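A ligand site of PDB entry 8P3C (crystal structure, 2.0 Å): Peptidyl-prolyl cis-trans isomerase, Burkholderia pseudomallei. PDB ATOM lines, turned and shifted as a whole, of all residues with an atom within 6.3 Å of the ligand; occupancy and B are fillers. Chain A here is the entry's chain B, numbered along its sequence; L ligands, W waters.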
ATOM      1  N   TYR A  46       7.710  12.650 -20.895  1.00  0.00           N
ATOM      2  CA  TYR A  46       6.518  11.768 -20.961  1.00  0.00           C
ATOM      3  C   TYR A  46       6.719  10.416 -20.265  1.00  0.00           C
ATOM      4  O   TYR A  46       7.861  10.028 -20.025  1.00  0.00           O
ATOM      5  CB  TYR A  46       6.120  11.458 -22.408  1.00  0.00           C
ATOM      6  CG  TYR A  46       7.030  10.540 -23.176  1.00  0.00           C
ATOM      7  CD1 TYR A  46       8.116  11.034 -23.887  1.00  0.00           C
ATOM      8  CD2 TYR A  46       6.812   9.174 -23.217  1.00  0.00           C
ATOM      9  CE1 TYR A  46       8.959  10.198 -24.599  1.00  0.00           C
ATOM     10  CE2 TYR A  46       7.642   8.320 -23.920  1.00  0.00           C
ATOM     11  CZ  TYR A  46       8.721   8.838 -24.611  1.00  0.00           C
ATOM     12  OH  TYR A  46       9.544   8.006 -25.323  1.00  0.00           O
ATOM     13  N   GLY A  48       4.642   6.419 -20.585  1.00  0.00           N
ATOM     14  CA  GLY A  48       3.564   5.678 -21.257  1.00  0.00           C
ATOM     15  C   GLY A  48       3.254   4.363 -20.548  1.00  0.00           C
ATOM     16  O   GLY A  48       4.194   3.677 -20.161  1.00  0.00           O
ATOM     17  N   PHE A  56       5.817   1.015 -20.558  1.00  0.00           N
ATOM     18  CA  PHE A  56       6.502   0.513 -21.771  1.00  0.00           C
ATOM     19  C   PHE A  56       7.616   1.478 -22.203  1.00  0.00           C
ATOM     20  O   PHE A  56       8.523   1.029 -22.906  1.00  0.00           O
ATOM     21  CB  PHE A  56       5.499   0.225 -22.882  1.00  0.00           C
ATOM     22  CG  PHE A  56       4.594   1.364 -23.287  1.00  0.00           C
ATOM     23  CD1 PHE A  56       5.084   2.421 -24.037  1.00  0.00           C
ATOM     24  CD2 PHE A  56       3.258   1.371 -22.944  1.00  0.00           C
ATOM     25  CE1 PHE A  56       4.254   3.464 -24.420  1.00  0.00           C
ATOM     26  CE2 PHE A  56       2.426   2.406 -23.333  1.00  0.00           C
ATOM     27  CZ  PHE A  56       2.924   3.449 -24.067  1.00  0.00           C
ATOM     28  N   ASP A  57       7.554   2.746 -21.763  1.00  0.00           N
ATOM     29  CA  ASP A  57       8.603   3.743 -22.126  1.00  0.00           C
ATOM     30  C   ASP A  57       8.475   5.035 -21.289  1.00  0.00           C
ATOM     31  O   ASP A  57       7.397   5.252 -20.730  1.00  0.00           O
ATOM     32  CB  ASP A  57       8.612   4.052 -23.629  1.00  0.00           C
ATOM     33  CG  ASP A  57       9.931   4.606 -24.144  1.00  0.00           C
ATOM     34  OD1 ASP A  57      10.939   4.447 -23.442  1.00  0.00           O
ATOM     35  OD2 ASP A  57       9.926   5.191 -25.234  1.00  0.00           O
ATOM     36  N   SER A  58       9.557   5.807 -21.210  1.00  0.00           N
ATOM     37  CA  SER A  58       9.562   7.107 -20.490  1.00  0.00           C
ATOM     38  C   SER A  58      10.677   8.016 -21.044  1.00  0.00           C
ATOM     39  O   SER A  58      11.716   7.502 -21.473  1.00  0.00           O
ATOM     40  CB  SER A  58       9.706   6.922 -19.009  1.00  0.00           C
ATOM     41  OG  SER A  58       9.827   8.188 -18.366  1.00  0.00           O
ATOM     42  N   PHE A  66      12.043  14.954 -25.469  1.00  0.00           N
ATOM     43  CA  PHE A  66      11.572  14.386 -26.746  1.00  0.00           C
ATOM     44  C   PHE A  66      10.981  15.527 -27.598  1.00  0.00           C
ATOM     45  O   PHE A  66      10.174  16.279 -27.077  1.00  0.00           O
ATOM     46  CB  PHE A  66      10.521  13.312 -26.496  1.00  0.00           C
ATOM     47  CG  PHE A  66       9.945  12.666 -27.734  1.00  0.00           C
ATOM     48  CD1 PHE A  66      10.653  11.691 -28.408  1.00  0.00           C
ATOM     49  CD2 PHE A  66       8.710  13.043 -28.227  1.00  0.00           C
ATOM     50  CE1 PHE A  66      10.126  11.096 -29.546  1.00  0.00           C
ATOM     51  CE2 PHE A  66       8.195  12.461 -29.366  1.00  0.00           C
ATOM     52  CZ  PHE A  66       8.904  11.488 -30.026  1.00  0.00           C
ATOM     53  N   GLY A  73       2.996  14.179 -38.610  1.00  0.00           N
ATOM     54  CA  GLY A  73       2.950  12.750 -38.769  1.00  0.00           C
ATOM     55  C   GLY A  73       4.218  12.025 -38.306  1.00  0.00           C
ATOM     56  O   GLY A  73       4.477  10.908 -38.779  1.00  0.00           O
ATOM     57  N   MET A  74       5.003  12.654 -37.453  1.00  0.00           N
ATOM     58  CA  MET A  74       6.237  12.021 -36.920  1.00  0.00           C
ATOM     59  C   MET A  74       5.864  11.057 -35.784  1.00  0.00           C
ATOM     60  O   MET A  74       6.681  10.182 -35.475  1.00  0.00           O
ATOM     61  CB  MET A  74       7.187  13.092 -36.400  1.00  0.00           C
ATOM     62  CG  MET A  74       7.680  14.050 -37.474  1.00  0.00           C
ATOM     63  SD  MET A  74       8.884  15.241 -36.850  1.00  0.00           S
ATOM     64  CE  MET A  74      10.330  14.188 -36.677  1.00  0.00           C
ATOM     65  N   VAL A  75       4.671  11.194 -35.215  1.00  0.00           N
ATOM     66  CA  VAL A  75       4.265  10.392 -34.030  1.00  0.00           C
ATOM     67  C   VAL A  75       2.852   9.827 -34.245  1.00  0.00           C
ATOM     68  O   VAL A  75       2.247  10.160 -35.256  1.00  0.00           O
ATOM     69  CB  VAL A  75       4.295  11.229 -32.737  1.00  0.00           C
ATOM     70  CG1 VAL A  75       5.708  11.673 -32.375  1.00  0.00           C
ATOM     71  CG2 VAL A  75       3.358  12.422 -32.821  1.00  0.00           C
ATOM     72  N   ILE A  76       2.385   9.025 -33.287  1.00  0.00           N
ATOM     73  CA  ILE A  76       1.010   8.442 -33.344  1.00  0.00           C
ATOM     74  C   ILE A  76      -0.031   9.558 -33.425  1.00  0.00           C
ATOM     75  O   ILE A  76       0.221  10.638 -32.901  1.00  0.00           O
ATOM     76  CB  ILE A  76       0.770   7.482 -32.161  1.00  0.00           C
ATOM     77  CG1 ILE A  76       0.953   8.143 -30.796  1.00  0.00           C
ATOM     78  CG2 ILE A  76       1.636   6.235 -32.298  1.00  0.00           C
ATOM     79  CD1 ILE A  76       0.639   7.229 -29.638  1.00  0.00           C
ATOM     80  N   LYS A  77      -1.184   9.277 -34.022  1.00  0.00           N
ATOM     81  CA  LYS A  77      -2.215  10.324 -34.274  1.00  0.00           C
ATOM     82  C   LYS A  77      -2.734  10.973 -32.973  1.00  0.00           C
ATOM     83  O   LYS A  77      -3.054  12.151 -33.038  1.00  0.00           O
ATOM     84  CB  LYS A  77      -3.348   9.738 -35.125  1.00  0.00           C
ATOM     85  CG  LYS A  77      -2.998   9.356 -36.556  1.00  0.00           C
ATOM     86  CD  LYS A  77      -4.034   8.441 -37.169  1.00  0.00           C
ATOM     87  CE  LYS A  77      -4.097   8.502 -38.674  1.00  0.00           C
ATOM     88  NZ  LYS A  77      -5.361   7.916 -39.195  1.00  0.00           N
ATOM     89  N   TRP A  79      -1.118  11.707 -30.355  1.00  0.00           N
ATOM     90  CA  TRP A  79      -0.143  12.743 -29.924  1.00  0.00           C
ATOM     91  C   TRP A  79      -0.241  13.984 -30.810  1.00  0.00           C
ATOM     92  O   TRP A  79      -0.249  15.082 -30.254  1.00  0.00           O
ATOM     93  CB  TRP A  79       1.273  12.176 -29.907  1.00  0.00           C
ATOM     94  CG  TRP A  79       1.703  11.587 -28.596  1.00  0.00           C
ATOM     95  CD1 TRP A  79       1.094  10.604 -27.880  1.00  0.00           C
ATOM     96  CD2 TRP A  79       2.871  11.955 -27.837  1.00  0.00           C
ATOM     97  NE1 TRP A  79       1.789  10.327 -26.734  1.00  0.00           N
ATOM     98  CE2 TRP A  79       2.890  11.150 -26.689  1.00  0.00           C
ATOM     99  CE3 TRP A  79       3.888  12.888 -28.037  1.00  0.00           C
ATOM    100  CZ2 TRP A  79       3.900  11.240 -25.736  1.00  0.00           C
ATOM    101  CZ3 TRP A  79       4.889  12.986 -27.091  1.00  0.00           C
ATOM    102  CH2 TRP A  79       4.886  12.170 -25.956  1.00  0.00           C
ATOM    103  N   GLY A 101      -3.460   4.983 -32.006  1.00  0.00           N
ATOM    104  CA  GLY A 101      -2.147   4.527 -31.514  1.00  0.00           C
ATOM    105  C   GLY A 101      -1.449   3.612 -32.528  1.00  0.00           C
ATOM    106  O   GLY A 101      -1.242   4.071 -33.652  1.00  0.00           O
ATOM    107  N   TYR A 102      -1.138   2.374 -32.151  1.00  0.00           N
ATOM    108  CA  TYR A 102      -0.375   1.428 -33.014  1.00  0.00           C
ATOM    109  C   TYR A 102      -1.311   0.381 -33.629  1.00  0.00           C
ATOM    110  O   TYR A 102      -0.812  -0.512 -34.328  1.00  0.00           O
ATOM    111  CB  TYR A 102       0.768   0.802 -32.217  1.00  0.00           C
ATOM    112  CG  TYR A 102       1.903   1.765 -31.952  1.00  0.00           C
ATOM    113  CD1 TYR A 102       2.732   2.182 -32.977  1.00  0.00           C
ATOM    114  CD2 TYR A 102       2.120   2.266 -30.685  1.00  0.00           C
ATOM    115  CE1 TYR A 102       3.763   3.072 -32.746  1.00  0.00           C
ATOM    116  CE2 TYR A 102       3.151   3.157 -30.440  1.00  0.00           C
ATOM    117  CZ  TYR A 102       3.969   3.568 -31.471  1.00  0.00           C
ATOM    118  OH  TYR A 102       4.989   4.454 -31.232  1.00  0.00           O
ATOM    119  N   ARG A 105      -1.017  -3.669 -35.544  1.00  0.00           N
ATOM    120  CA  ARG A 105       0.417  -4.007 -35.664  1.00  0.00           C
ATOM    121  C   ARG A 105       1.086  -4.075 -34.290  1.00  0.00           C
ATOM    122  O   ARG A 105       2.008  -4.869 -34.133  1.00  0.00           O
ATOM    123  CB  ARG A 105       1.160  -2.949 -36.482  1.00  0.00           C
ATOM    124  CG  ARG A 105       0.553  -2.630 -37.840  1.00  0.00           C
ATOM    125  CD  ARG A 105       1.518  -1.821 -38.687  1.00  0.00           C
ATOM    126  NE  ARG A 105       1.924  -0.551 -38.093  1.00  0.00           N
ATOM    127  CZ  ARG A 105       1.166   0.186 -37.294  1.00  0.00           C
ATOM    128  NH1 ARG A 105       0.118   0.837 -37.775  1.00  0.00           N
ATOM    129  NH2 ARG A 105       1.457   0.280 -36.008  1.00  0.00           N
ATOM    130  N   ALA A 107       3.651  -2.641 -31.320  1.00  0.00           N
ATOM    131  CA  ALA A 107       4.993  -2.012 -31.438  1.00  0.00           C
ATOM    132  C   ALA A 107       6.075  -2.825 -30.734  1.00  0.00           C
ATOM    133  O   ALA A 107       5.950  -3.038 -29.530  1.00  0.00           O
ATOM    134  CB  ALA A 107       4.977  -0.595 -30.936  1.00  0.00           C
ATOM    135  N   GLY A 108       7.069  -3.301 -31.486  1.00  0.00           N
ATOM    136  CA  GLY A 108       8.233  -3.988 -30.890  1.00  0.00           C
ATOM    137  C   GLY A 108       7.986  -5.289 -30.162  1.00  0.00           C
ATOM    138  O   GLY A 108       8.946  -5.856 -29.638  1.00  0.00           O
ATOM    139  N   VAL A 110       6.267  -5.338 -27.531  1.00  0.00           N
ATOM    140  CA  VAL A 110       6.021  -4.882 -26.129  1.00  0.00           C
ATOM    141  C   VAL A 110       4.578  -4.355 -26.015  1.00  0.00           C
ATOM    142  O   VAL A 110       3.916  -4.687 -25.016  1.00  0.00           O
ATOM    143  CB  VAL A 110       7.057  -3.841 -25.686  1.00  0.00           C
ATOM    144  CG1 VAL A 110       6.859  -3.397 -24.249  1.00  0.00           C
ATOM    145  CG2 VAL A 110       8.487  -4.321 -25.919  1.00  0.00           C
ATOM    146  N   ILE A 111       4.136  -3.538 -26.965  1.00  0.00           N
ATOM    147  CA  ILE A 111       2.725  -3.060 -26.988  1.00  0.00           C
ATOM    148  C   ILE A 111       1.922  -4.035 -27.861  1.00  0.00           C
ATOM    149  O   ILE A 111       2.229  -4.131 -29.044  1.00  0.00           O
ATOM    150  CB  ILE A 111       2.611  -1.612 -27.518  1.00  0.00           C
ATOM    151  CG1 ILE A 111       3.181  -0.574 -26.547  1.00  0.00           C
ATOM    152  CG2 ILE A 111       1.183  -1.301 -27.922  1.00  0.00           C
ATOM    153  CD1 ILE A 111       3.202   0.826 -27.110  1.00  0.00           C
ATOM    154  N   LEU A 117      -3.719   3.075 -24.874  1.00  0.00           N
ATOM    155  CA  LEU A 117      -2.483   3.553 -24.263  1.00  0.00           C
ATOM    156  C   LEU A 117      -2.810   4.746 -23.377  1.00  0.00           C
ATOM    157  O   LEU A 117      -3.676   5.568 -23.722  1.00  0.00           O
ATOM    158  CB  LEU A 117      -1.469   3.983 -25.342  1.00  0.00           C
ATOM    159  CG  LEU A 117      -1.187   3.015 -26.493  1.00  0.00           C
ATOM    160  CD1 LEU A 117      -0.232   3.639 -27.541  1.00  0.00           C
ATOM    161  CD2 LEU A 117      -0.650   1.672 -26.003  1.00  0.00           C
ATOM    162  N   PHE A 119      -0.876   7.991 -21.526  1.00  0.00           N
ATOM    163  CA  PHE A 119       0.378   8.762 -21.387  1.00  0.00           C
ATOM    164  C   PHE A 119       0.182  10.010 -20.530  1.00  0.00           C
ATOM    165  O   PHE A 119      -0.908  10.582 -20.590  1.00  0.00           O
ATOM    166  CB  PHE A 119       0.860   9.288 -22.743  1.00  0.00           C
ATOM    167  CG  PHE A 119       1.393   8.301 -23.747  1.00  0.00           C
ATOM    168  CD1 PHE A 119       0.529   7.626 -24.607  1.00  0.00           C
ATOM    169  CD2 PHE A 119       2.758   8.093 -23.900  1.00  0.00           C
ATOM    170  CE1 PHE A 119       1.020   6.745 -25.557  1.00  0.00           C
ATOM    171  CE2 PHE A 119       3.237   7.207 -24.842  1.00  0.00           C
ATOM    172  CZ  PHE A 119       2.373   6.536 -25.674  1.00  0.00           C
HETATM  173  N1  LIG L   1       6.225   6.854 -28.450  1.00  0.00           N
HETATM  174  N2  LIG L   1       6.363   7.179 -34.856  1.00  0.00           N
HETATM  175  C1  LIG L   1       7.377   3.004 -28.006  1.00  0.00           C
HETATM  176  C2  LIG L   1       7.193   4.333 -28.679  1.00  0.00           C
HETATM  177  C3  LIG L   1       5.179   7.335 -29.376  1.00  0.00           C
HETATM  178  C4  LIG L   1       5.525   7.473 -30.868  1.00  0.00           C
HETATM  179  C5  LIG L   1       7.249   7.371 -32.589  1.00  0.00           C
HETATM  180  C6  LIG L   1       9.351   6.109 -31.801  1.00  0.00           C
HETATM  181  C7  LIG L   1      10.426   4.095 -30.257  1.00  0.00           C
HETATM  182  C8  LIG L   1       9.251   4.787 -32.190  1.00  0.00           C
HETATM  183  C9  LIG L   1       5.899   6.477 -36.034  1.00  0.00           C
HETATM  184  C10 LIG L   1       1.749   6.822 -36.733  1.00  0.00           C
HETATM  185  C11 LIG L   1       2.560   7.796 -37.224  1.00  0.00           C
HETATM  186  C12 LIG L   1       3.913   7.701 -37.004  1.00  0.00           C
HETATM  187  C13 LIG L   1       5.710   9.655 -28.607  1.00  0.00           C
HETATM  188  C14 LIG L   1       7.324   7.788 -28.175  1.00  0.00           C
HETATM  189  C15 LIG L   1       8.600   1.574 -26.503  1.00  0.00           C
HETATM  190  F1  LIG L   1       7.887  -0.630 -26.187  1.00  0.00           F
HETATM  191  C16 LIG L   1       7.722   0.573 -26.790  1.00  0.00           C
HETATM  192  C17 LIG L   1       6.682   0.722 -27.646  1.00  0.00           C
HETATM  193  C18 LIG L   1       6.513   1.961 -28.261  1.00  0.00           C
HETATM  194  S1  LIG L   1       6.118   5.418 -27.747  1.00  0.00           S
HETATM  195  O1  LIG L   1       6.674   5.522 -26.431  1.00  0.00           O
HETATM  196  N3  LIG L   1       6.718   7.036 -31.279  1.00  0.00           N
HETATM  197  C19 LIG L   1       8.774   7.210 -32.657  1.00  0.00           C
HETATM  198  C20 LIG L   1      10.019   6.395 -30.620  1.00  0.00           C
HETATM  199  C21 LIG L   1      10.561   5.386 -29.837  1.00  0.00           C
HETATM  200  F2  LIG L   1      10.951   3.108 -29.497  1.00  0.00           F
HETATM  201  C22 LIG L   1       9.791   3.762 -31.420  1.00  0.00           C
HETATM  202  C23 LIG L   1       6.584   6.551 -33.694  1.00  0.00           C
HETATM  203  C24 LIG L   1       4.424   6.630 -36.300  1.00  0.00           C
HETATM  204  C25 LIG L   1       3.520   5.704 -35.847  1.00  0.00           C
HETATM  205  N4  LIG L   1       2.203   5.774 -36.044  1.00  0.00           N
HETATM  206  O2  LIG L   1       6.248   5.388 -33.498  1.00  0.00           O
HETATM  207  O3  LIG L   1       4.715   7.972 -31.658  1.00  0.00           O
HETATM  208  C26 LIG L   1       4.606   8.635 -28.823  1.00  0.00           C
HETATM  209  C27 LIG L   1       6.764   9.103 -27.660  1.00  0.00           C
HETATM  210  O4  LIG L   1       4.787   4.915 -27.927  1.00  0.00           O
HETATM  211  C28 LIG L   1       8.419   2.800 -27.130  1.00  0.00           C
HETATM  212  O   HOH W   1       0.529   3.519 -35.882  1.00  0.00           O
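An oxygen (O1) of the ligand lies close to the side-chain carboxylate of Asp 57. Tyr 46 touches the ligand (OH to C14, 3.6 Å). Phe 56 touches the ligand (O to C15, 3.6 Å). Phe 66 touches the ligand. O of Gly 73 touches C12 of the ligand, at 3.7 Å. Val 75 touches the ligand (O to C11, 3.1 Å). CE2 of Trp 79 touches C26 of the ligand, at 3.7 Å. Ala 107 touches the ligand. Val 110 touches the ligand (CB to F1, 3.4 Å). Ile 111 touches the ligand. Phe 119 touches the ligand (CZ to O4, 3.7 Å). Hydrophobic or aromatic side chains that line the ligand: Tyr 46, Phe 56, Phe 66, Val 75, Ile 76, Trp 79, Tyr 102, Ala 107, Val 110, Ile 111 and Phe 119. The nearest printed residue that does not touch the ligand is Gly 101 (4.5 Å).
O of Tyr 102 sits at hydrogen-bond distance from NH2 of Arg 105, at 2.9 Å. The side-chain carboxylate of Asp 57 lies within hydrogen-bond range of the side-chain hydroxyl of Tyr 46, 2.8 Å away. O of Tyr 46 lies within hydrogen-bond range of OG of Ser 58, 3.2 Å away. The backbone NH of Phe 56 lies within hydrogen-bond range of the backbone carbonyl oxygen of Gly 48. The backbone carbonyl oxygen (O) of Asp 57 sits at hydrogen-bond distance from the backbone NH (N) of Gly 48.
An oxygen (O3) of the ligand is in hydrogen-bond range of the backbone NH of Ile 76 (3.0 Å). OH of Tyr 102 sits at hydrogen-bond distance from O2 of the ligand (2.8 Å). The backbone carbonyl oxygen (O) of Met 74 sits at hydrogen-bond distance from a nitrogen (N2) of the ligand (3.1 Å).
Water W1 lies within hydrogen-bond range of N4 of the ligand (2.8 Å), O of Gly 101 (2.9 Å) and NH1 of Arg 105 (3.3 Å).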
